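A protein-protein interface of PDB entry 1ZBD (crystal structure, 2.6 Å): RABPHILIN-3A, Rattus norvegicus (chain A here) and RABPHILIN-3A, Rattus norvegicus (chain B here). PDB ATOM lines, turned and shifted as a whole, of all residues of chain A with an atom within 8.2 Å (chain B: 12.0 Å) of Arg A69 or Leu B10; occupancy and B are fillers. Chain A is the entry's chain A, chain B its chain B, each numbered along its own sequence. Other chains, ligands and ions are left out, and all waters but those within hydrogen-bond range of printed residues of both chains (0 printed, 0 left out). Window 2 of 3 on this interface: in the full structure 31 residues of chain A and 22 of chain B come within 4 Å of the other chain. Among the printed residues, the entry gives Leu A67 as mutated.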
ATOM      1  N   SER A  39      28.222 -13.752   5.058  1.00  0.00           N
ATOM      2  CA  SER A  39      27.566 -14.035   3.789  1.00  0.00           C
ATOM      3  C   SER A  39      28.237 -13.239   2.677  1.00  0.00           C
ATOM      4  O   SER A  39      28.506 -12.045   2.829  1.00  0.00           O
ATOM      5  CB  SER A  39      26.076 -13.683   3.860  1.00  0.00           C
ATOM      6  OG  SER A  39      25.405 -14.060   2.665  1.00  0.00           O
ATOM      7  N   THR A  40      28.510 -13.918   1.565  1.00  0.00           N
ATOM      8  CA  THR A  40      29.163 -13.313   0.412  1.00  0.00           C
ATOM      9  C   THR A  40      28.254 -12.326  -0.321  1.00  0.00           C
ATOM     10  O   THR A  40      27.063 -12.581  -0.521  1.00  0.00           O
ATOM     11  CB  THR A  40      29.619 -14.402  -0.574  1.00  0.00           C
ATOM     12  OG1 THR A  40      30.522 -15.295   0.088  1.00  0.00           O
ATOM     13  CG2 THR A  40      30.308 -13.782  -1.782  1.00  0.00           C
ATOM     14  N   VAL A  41      28.826 -11.198  -0.730  1.00  0.00           N
ATOM     15  CA  VAL A  41      28.064 -10.180  -1.440  1.00  0.00           C
ATOM     16  C   VAL A  41      28.172 -10.358  -2.954  1.00  0.00           C
ATOM     17  O   VAL A  41      29.129  -9.902  -3.579  1.00  0.00           O
ATOM     18  CB  VAL A  41      28.547  -8.761  -1.064  1.00  0.00           C
ATOM     19  CG1 VAL A  41      27.702  -7.711  -1.774  1.00  0.00           C
ATOM     20  CG2 VAL A  41      28.475  -8.577   0.443  1.00  0.00           C
ATOM     21  N   GLY A  42      27.178 -11.021  -3.538  1.00  0.00           N
ATOM     22  CA  GLY A  42      27.185 -11.245  -4.971  1.00  0.00           C
ATOM     23  C   GLY A  42      28.156 -12.339  -5.369  1.00  0.00           C
ATOM     24  O   GLY A  42      27.827 -13.521  -5.304  1.00  0.00           O
ATOM     25  N   ALA A  65      27.202 -16.181  -4.247  1.00  0.00           N
ATOM     26  CA  ALA A  65      26.307 -15.969  -3.115  1.00  0.00           C
ATOM     27  C   ALA A  65      25.151 -16.946  -3.253  1.00  0.00           C
ATOM     28  O   ALA A  65      24.569 -17.073  -4.325  1.00  0.00           O
ATOM     29  CB  ALA A  65      25.784 -14.542  -3.114  1.00  0.00           C
ATOM     30  N   GLY A  66      24.824 -17.636  -2.166  1.00  0.00           N
ATOM     31  CA  GLY A  66      23.743 -18.602  -2.211  1.00  0.00           C
ATOM     32  C   GLY A  66      22.354 -18.001  -2.101  1.00  0.00           C
ATOM     33  O   GLY A  66      21.392 -18.563  -2.623  1.00  0.00           O
ATOM     34  N   LEU A  67      22.248 -16.858  -1.428  1.00  0.00           N
ATOM     35  CA  LEU A  67      20.961 -16.196  -1.243  1.00  0.00           C
ATOM     36  C   LEU A  67      20.267 -15.858  -2.556  1.00  0.00           C
ATOM     37  O   LEU A  67      20.887 -15.356  -3.493  1.00  0.00           O
ATOM     38  CB  LEU A  67      21.137 -14.931  -0.400  1.00  0.00           C
ATOM     39  CG  LEU A  67      21.589 -15.183   1.044  1.00  0.00           C
ATOM     40  CD1 LEU A  67      21.847 -13.862   1.752  1.00  0.00           C
ATOM     41  CD2 LEU A  67      20.520 -15.985   1.773  1.00  0.00           C
ATOM     42  N   GLU A  68      18.966 -16.132  -2.602  1.00  0.00           N
ATOM     43  CA  GLU A  68      18.154 -15.884  -3.787  1.00  0.00           C
ATOM     44  C   GLU A  68      18.230 -14.429  -4.228  1.00  0.00           C
ATOM     45  O   GLU A  68      17.787 -14.074  -5.319  1.00  0.00           O
ATOM     46  CB  GLU A  68      16.699 -16.258  -3.502  1.00  0.00           C
ATOM     47  CG  GLU A  68      15.808 -16.308  -4.734  1.00  0.00           C
ATOM     48  CD  GLU A  68      14.383 -16.706  -4.394  1.00  0.00           C
ATOM     49  OE1 GLU A  68      14.186 -17.805  -3.830  1.00  0.00           O
ATOM     50  OE2 GLU A  68      13.458 -15.917  -4.687  1.00  0.00           O
ATOM     51  N   ARG A  69      18.806 -13.593  -3.377  1.00  0.00           N
ATOM     52  CA  ARG A  69      18.934 -12.176  -3.666  1.00  0.00           C
ATOM     53  C   ARG A  69      19.817 -11.861  -4.877  1.00  0.00           C
ATOM     54  O   ARG A  69      19.455 -11.033  -5.712  1.00  0.00           O
ATOM     55  CB  ARG A  69      19.482 -11.452  -2.435  1.00  0.00           C
ATOM     56  CG  ARG A  69      19.619  -9.961  -2.629  1.00  0.00           C
ATOM     57  CD  ARG A  69      20.196  -9.286  -1.407  1.00  0.00           C
ATOM     58  NE  ARG A  69      20.178  -7.835  -1.563  1.00  0.00           N
ATOM     59  CZ  ARG A  69      20.662  -6.980  -0.670  1.00  0.00           C
ATOM     60  NH1 ARG A  69      21.207  -7.429   0.453  1.00  0.00           N
ATOM     61  NH2 ARG A  69      20.595  -5.673  -0.898  1.00  0.00           N
ATOM     62  N   TYR A  70      20.965 -12.526  -4.978  1.00  0.00           N
ATOM     63  CA  TYR A  70      21.898 -12.271  -6.076  1.00  0.00           C
ATOM     64  C   TYR A  70      21.826 -13.244  -7.251  1.00  0.00           C
ATOM     65  O   TYR A  70      22.772 -13.352  -8.029  1.00  0.00           O
ATOM     66  CB  TYR A  70      23.330 -12.261  -5.543  1.00  0.00           C
ATOM     67  CG  TYR A  70      23.551 -11.379  -4.328  1.00  0.00           C
ATOM     68  CD1 TYR A  70      23.716  -9.999  -4.463  1.00  0.00           C
ATOM     69  CD2 TYR A  70      23.626 -11.928  -3.046  1.00  0.00           C
ATOM     70  CE1 TYR A  70      23.953  -9.188  -3.353  1.00  0.00           C
ATOM     71  CE2 TYR A  70      23.867 -11.125  -1.928  1.00  0.00           C
ATOM     72  CZ  TYR A  70      24.030  -9.757  -2.090  1.00  0.00           C
ATOM     73  OH  TYR A  70      24.270  -8.956  -0.995  1.00  0.00           O
ATOM     74  N   ARG A  71      20.704 -13.942  -7.384  1.00  0.00           N
ATOM     75  CA  ARG A  71      20.519 -14.913  -8.458  1.00  0.00           C
ATOM     76  C   ARG A  71      20.938 -14.394  -9.839  1.00  0.00           C
ATOM     77  O   ARG A  71      21.776 -15.001 -10.511  1.00  0.00           O
ATOM     78  CB  ARG A  71      19.051 -15.345  -8.524  1.00  0.00           C
ATOM     79  CG  ARG A  71      18.813 -16.637  -9.295  1.00  0.00           C
ATOM     80  CD  ARG A  71      18.794 -17.819  -8.341  1.00  0.00           C
ATOM     81  NE  ARG A  71      19.889 -17.743  -7.382  1.00  0.00           N
ATOM     82  CZ  ARG A  71      19.940 -18.434  -6.249  1.00  0.00           C
ATOM     83  NH1 ARG A  71      18.956 -19.263  -5.926  1.00  0.00           N
ATOM     84  NH2 ARG A  71      20.969 -18.281  -5.428  1.00  0.00           N
ATOM     85  N   THR A  72      20.348 -13.276 -10.260  1.00  0.00           N
ATOM     86  CA  THR A  72      20.631 -12.697 -11.573  1.00  0.00           C
ATOM     87  C   THR A  72      22.096 -12.363 -11.838  1.00  0.00           C
ATOM     88  O   THR A  72      22.609 -12.623 -12.933  1.00  0.00           O
ATOM     89  CB  THR A  72      19.776 -11.432 -11.822  1.00  0.00           C
ATOM     90  OG1 THR A  72      18.405 -11.812 -11.998  1.00  0.00           O
ATOM     91  CG2 THR A  72      20.247 -10.699 -13.075  1.00  0.00           C
ATOM     92  N   ILE A  73      22.773 -11.786 -10.853  1.00  0.00           N
ATOM     93  CA  ILE A  73      24.174 -11.445 -11.036  1.00  0.00           C
ATOM     94  C   ILE A  73      25.098 -12.668 -11.008  1.00  0.00           C
ATOM     95  O   ILE A  73      26.086 -12.715 -11.742  1.00  0.00           O
ATOM     96  CB  ILE A  73      24.645 -10.414  -9.978  1.00  0.00           C
ATOM     97  CG1 ILE A  73      26.164 -10.266 -10.042  1.00  0.00           C
ATOM     98  CG2 ILE A  73      24.197 -10.830  -8.594  1.00  0.00           C
ATOM     99  CD1 ILE A  73      26.728  -9.330  -8.999  1.00  0.00           C
ATOM    100  N   THR A  74      24.777 -13.660 -10.178  1.00  0.00           N
ATOM    101  CA  THR A  74      25.611 -14.858 -10.093  1.00  0.00           C
ATOM    102  C   THR A  74      25.418 -15.783 -11.288  1.00  0.00           C
ATOM    103  O   THR A  74      26.371 -16.394 -11.766  1.00  0.00           O
ATOM    104  CB  THR A  74      25.329 -15.670  -8.806  1.00  0.00           C
ATOM    105  OG1 THR A  74      23.925 -15.929  -8.702  1.00  0.00           O
ATOM    106  CG2 THR A  74      25.791 -14.908  -7.576  1.00  0.00           C
ATOM    107  N   GLU B   8      13.683  -7.733  -8.851  1.00  0.00           N
ATOM    108  CA  GLU B   8      15.035  -7.627  -8.227  1.00  0.00           C
ATOM    109  C   GLU B   8      14.989  -6.960  -6.858  1.00  0.00           C
ATOM    110  O   GLU B   8      14.053  -7.167  -6.086  1.00  0.00           O
ATOM    111  CB  GLU B   8      15.978  -6.831  -9.131  1.00  0.00           C
ATOM    112  CG  GLU B   8      16.346  -7.523 -10.432  1.00  0.00           C
ATOM    113  CD  GLU B   8      17.412  -6.763 -11.202  1.00  0.00           C
ATOM    114  OE1 GLU B   8      18.524  -6.586 -10.653  1.00  0.00           O
ATOM    115  OE2 GLU B   8      17.137  -6.345 -12.350  1.00  0.00           O
ATOM    116  N   GLU B   9      16.015  -6.164  -6.569  1.00  0.00           N
ATOM    117  CA  GLU B   9      16.127  -5.450  -5.302  1.00  0.00           C
ATOM    118  C   GLU B   9      17.091  -4.278  -5.427  1.00  0.00           C
ATOM    119  O   GLU B   9      17.765  -4.119  -6.446  1.00  0.00           O
ATOM    120  CB  GLU B   9      16.624  -6.384  -4.198  1.00  0.00           C
ATOM    121  CG  GLU B   9      15.592  -7.375  -3.702  1.00  0.00           C
ATOM    122  CD  GLU B   9      16.136  -8.275  -2.615  1.00  0.00           C
ATOM    123  OE1 GLU B   9      16.695  -7.742  -1.631  1.00  0.00           O
ATOM    124  OE2 GLU B   9      16.002  -9.511  -2.743  1.00  0.00           O
ATOM    125  N   LEU B  10      17.150  -3.461  -4.380  1.00  0.00           N
ATOM    126  CA  LEU B  10      18.041  -2.308  -4.364  1.00  0.00           C
ATOM    127  C   LEU B  10      19.443  -2.783  -4.002  1.00  0.00           C
ATOM    128  O   LEU B  10      19.663  -3.975  -3.787  1.00  0.00           O
ATOM    129  CB  LEU B  10      17.557  -1.270  -3.342  1.00  0.00           C
ATOM    130  CG  LEU B  10      16.166  -0.650  -3.549  1.00  0.00           C
ATOM    131  CD1 LEU B  10      15.867   0.331  -2.418  1.00  0.00           C
ATOM    132  CD2 LEU B  10      16.103   0.060  -4.900  1.00  0.00           C
ATOM    133  N   THR B  11      20.387  -1.850  -3.934  1.00  0.00           N
ATOM    134  CA  THR B  11      21.763  -2.189  -3.602  1.00  0.00           C
ATOM    135  C   THR B  11      22.553  -0.946  -3.199  1.00  0.00           C
ATOM    136  O   THR B  11      22.918  -0.125  -4.043  1.00  0.00           O
ATOM    137  CB  THR B  11      22.458  -2.870  -4.796  1.00  0.00           C
ATOM    138  OG1 THR B  11      21.799  -4.108  -5.092  1.00  0.00           O
ATOM    139  CG2 THR B  11      23.912  -3.141  -4.478  1.00  0.00           C
ATOM    140  N   ASP B  12      22.817  -0.821  -1.903  1.00  0.00           N
ATOM    141  CA  ASP B  12      23.553   0.319  -1.364  1.00  0.00           C
ATOM    142  C   ASP B  12      24.960   0.457  -1.949  1.00  0.00           C
ATOM    143  O   ASP B  12      25.130   0.827  -3.112  1.00  0.00           O
ATOM    144  CB  ASP B  12      23.627   0.206   0.165  1.00  0.00           C
ATOM    145  CG  ASP B  12      24.119  -1.157   0.628  1.00  0.00           C
ATOM    146  N   GLU B  13      25.962   0.170  -1.123  1.00  0.00           N
ATOM    147  CA  GLU B  13      27.359   0.240  -1.530  1.00  0.00           C
ATOM    148  C   GLU B  13      27.799  -1.134  -2.009  1.00  0.00           C
ATOM    149  O   GLU B  13      28.939  -1.318  -2.434  1.00  0.00           O
ATOM    150  CB  GLU B  13      28.240   0.658  -0.353  1.00  0.00           C
ATOM    151  CG  GLU B  13      28.070  -0.232   0.873  1.00  0.00           C
ATOM    152  CD  GLU B  13      29.209  -0.095   1.862  1.00  0.00           C
ATOM    153  OE1 GLU B  13      30.329  -0.560   1.550  1.00  0.00           O
ATOM    154  OE2 GLU B  13      28.985   0.480   2.951  1.00  0.00           O
ATOM    155  N   GLU B  14      26.893  -2.103  -1.919  1.00  0.00           N
ATOM    156  CA  GLU B  14      27.186  -3.463  -2.347  1.00  0.00           C
ATOM    157  C   GLU B  14      27.781  -3.413  -3.746  1.00  0.00           C
ATOM    158  O   GLU B  14      28.766  -4.091  -4.034  1.00  0.00           O
ATOM    159  CB  GLU B  14      25.909  -4.298  -2.359  1.00  0.00           C
ATOM    160  CG  GLU B  14      25.173  -4.329  -1.031  1.00  0.00           C
ATOM    161  CD  GLU B  14      23.788  -4.929  -1.154  1.00  0.00           C
ATOM    162  OE1 GLU B  14      22.945  -4.337  -1.866  1.00  0.00           O
ATOM    163  OE2 GLU B  14      23.544  -5.993  -0.544  1.00  0.00           O
ATOM    164  N   LYS B  15      27.178  -2.600  -4.610  1.00  0.00           N
ATOM    165  CA  LYS B  15      27.659  -2.442  -5.977  1.00  0.00           C
ATOM    166  C   LYS B  15      29.149  -2.130  -5.932  1.00  0.00           C
ATOM    167  O   LYS B  15      29.947  -2.710  -6.667  1.00  0.00           O
ATOM    168  CB  LYS B  15      26.932  -1.290  -6.674  1.00  0.00           C
ATOM    169  CG  LYS B  15      25.433  -1.467  -6.818  1.00  0.00           C
ATOM    170  CD  LYS B  15      24.823  -0.294  -7.567  1.00  0.00           C
ATOM    171  CE  LYS B  15      23.327  -0.469  -7.759  1.00  0.00           C
ATOM    172  NZ  LYS B  15      22.753   0.622  -8.594  1.00  0.00           N
ATOM    173  N   GLU B  16      29.505  -1.200  -5.054  1.00  0.00           N
ATOM    174  CA  GLU B  16      30.882  -0.766  -4.872  1.00  0.00           C
ATOM    175  C   GLU B  16      31.791  -1.960  -4.565  1.00  0.00           C
ATOM    176  O   GLU B  16      32.924  -2.031  -5.043  1.00  0.00           O
ATOM    177  CB  GLU B  16      30.928   0.257  -3.732  1.00  0.00           C
ATOM    178  CG  GLU B  16      32.272   0.908  -3.472  1.00  0.00           C
ATOM    179  CD  GLU B  16      32.218   1.872  -2.296  1.00  0.00           C
ATOM    180  OE1 GLU B  16      31.454   2.860  -2.368  1.00  0.00           O
ATOM    181  OE2 GLU B  16      32.934   1.637  -1.297  1.00  0.00           O
ATOM    182  N   ILE B  17      31.278  -2.898  -3.773  1.00  0.00           N
ATOM    183  CA  ILE B  17      32.022  -4.094  -3.386  1.00  0.00           C
ATOM    184  C   ILE B  17      32.135  -5.082  -4.549  1.00  0.00           C
ATOM    185  O   ILE B  17      33.149  -5.770  -4.699  1.00  0.00           O
ATOM    186  CB  ILE B  17      31.329  -4.812  -2.211  1.00  0.00           C
ATOM    187  CG1 ILE B  17      31.038  -3.810  -1.089  1.00  0.00           C
ATOM    188  CG2 ILE B  17      32.208  -5.947  -1.702  1.00  0.00           C
ATOM    189  CD1 ILE B  17      30.238  -4.386   0.059  1.00  0.00           C
ATOM    190  N   ILE B  18      31.082  -5.143  -5.362  1.00  0.00           N
ATOM    191  CA  ILE B  18      31.029  -6.038  -6.510  1.00  0.00           C
ATOM    192  C   ILE B  18      31.829  -5.518  -7.697  1.00  0.00           C
ATOM    193  O   ILE B  18      32.595  -6.261  -8.315  1.00  0.00           O
ATOM    194  CB  ILE B  18      29.566  -6.272  -6.961  1.00  0.00           C
ATOM    195  CG1 ILE B  18      28.846  -7.149  -5.931  1.00  0.00           C
ATOM    196  CG2 ILE B  18      29.534  -6.919  -8.345  1.00  0.00           C
ATOM    197  CD1 ILE B  18      27.408  -7.450  -6.276  1.00  0.00           C
ATOM    198  N   ASN B  19      31.646  -4.243  -8.018  1.00  0.00           N
ATOM    199  CA  ASN B  19      32.357  -3.644  -9.138  1.00  0.00           C
ATOM    200  C   ASN B  19      33.856  -3.872  -9.017  1.00  0.00           C
ATOM    201  O   ASN B  19      34.541  -4.008 -10.027  1.00  0.00           O
ATOM    202  CB  ASN B  19      32.056  -2.148  -9.226  1.00  0.00           C
ATOM    203  CG  ASN B  19      30.590  -1.864  -9.500  1.00  0.00           C
ATOM    204  OD1 ASN B  19      29.989  -2.449 -10.404  1.00  0.00           O
ATOM    205  ND2 ASN B  19      30.008  -0.956  -8.723  1.00  0.00           N
ATOM    206  N   PRO B 130      27.514  -2.197 -12.775  1.00  0.00           N
ATOM    207  CA  PRO B 130      26.285  -1.449 -12.477  1.00  0.00           C
ATOM    208  C   PRO B 130      26.548  -0.183 -11.658  1.00  0.00           C
ATOM    209  O   PRO B 130      26.628  -0.233 -10.430  1.00  0.00           O
ATOM    210  CB  PRO B 130      25.442  -2.469 -11.711  1.00  0.00           C
ATOM    211  CG  PRO B 130      26.477  -3.241 -10.955  1.00  0.00           C
ATOM    212  CD  PRO B 130      27.547  -3.462 -12.015  1.00  0.00           C
ATOM    213  N   MET B 131      26.679   0.949 -12.347  1.00  0.00           N
ATOM    214  CA  MET B 131      26.940   2.227 -11.689  1.00  0.00           C
ATOM    215  C   MET B 131      25.798   2.647 -10.763  1.00  0.00           C
ATOM    216  O   MET B 131      24.768   1.939 -10.730  1.00  0.00           O
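NE of Arg A69 lies within salt-bridge range of OE1 of Glu B9, at 3.5 Å. The backbone carbonyl oxygen of Leu B10 sits at hydrogen-bond distance from the guanidinium group of Arg A69, 3.5 Å away. The guanidinium group (NH2) of Arg A69 is in salt-bridge range of the side-chain carboxylate (OE1) of Glu B14, 2.9 Å away. OE2 of Glu B14 lies within hydrogen-bond range of OH of Tyr A70 (3.1 Å).
The side-chain hydroxyl of Thr A74 is in hydrogen-bond range of the backbone carbonyl oxygen of Tyr A70 (2.9 Å). The side-chain carboxylate (OE1) of Glu B14 lies close to the side-chain hydroxyl (OG1) of Thr B11, 3.4 Å away.
Glu B14 touches Val A41. O of Val A41 touches CG1 of Ile B18, at 3.6 Å. CD1 of Ile A73 touches CD1 of Ile B18, at 3.4 Å.
No residue of chain B comes within 4 Å of Gly A66. No residue of chain B comes within 4 Å of Leu A67. Of chain B, only Glu B9, Leu B10 and Glu B14 come within 4 Å of Arg A69. No residue of chain B comes within 4 Å of Arg A71. Of the printed residues of chain A, Glu B9 touches Arg A69. Of chain A, only Arg A69 comes within 4 Å of Leu B10. Of the printed residues of chain A, Ile B18 touches Val A41 and Ile A73. The nearest residue of chain A that does not touch Leu B10 is Tyr A70 (6.8 Å). The nearest printed residue of chain B that does not touch Val A41 is Ile B17 (4.6 Å).
Printed residues of chain B that touch a printed residue of chain A: Glu B9, Leu B10, Glu B14 and Ile B18. Hydrophobic or aromatic side chains of chain B that line the printed part of chain A: Ile B18. Of the 14 printed residues of chain A, 4 touch a printed residue of chain B. Among the printed residues, 7 pairs touch across the chains.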
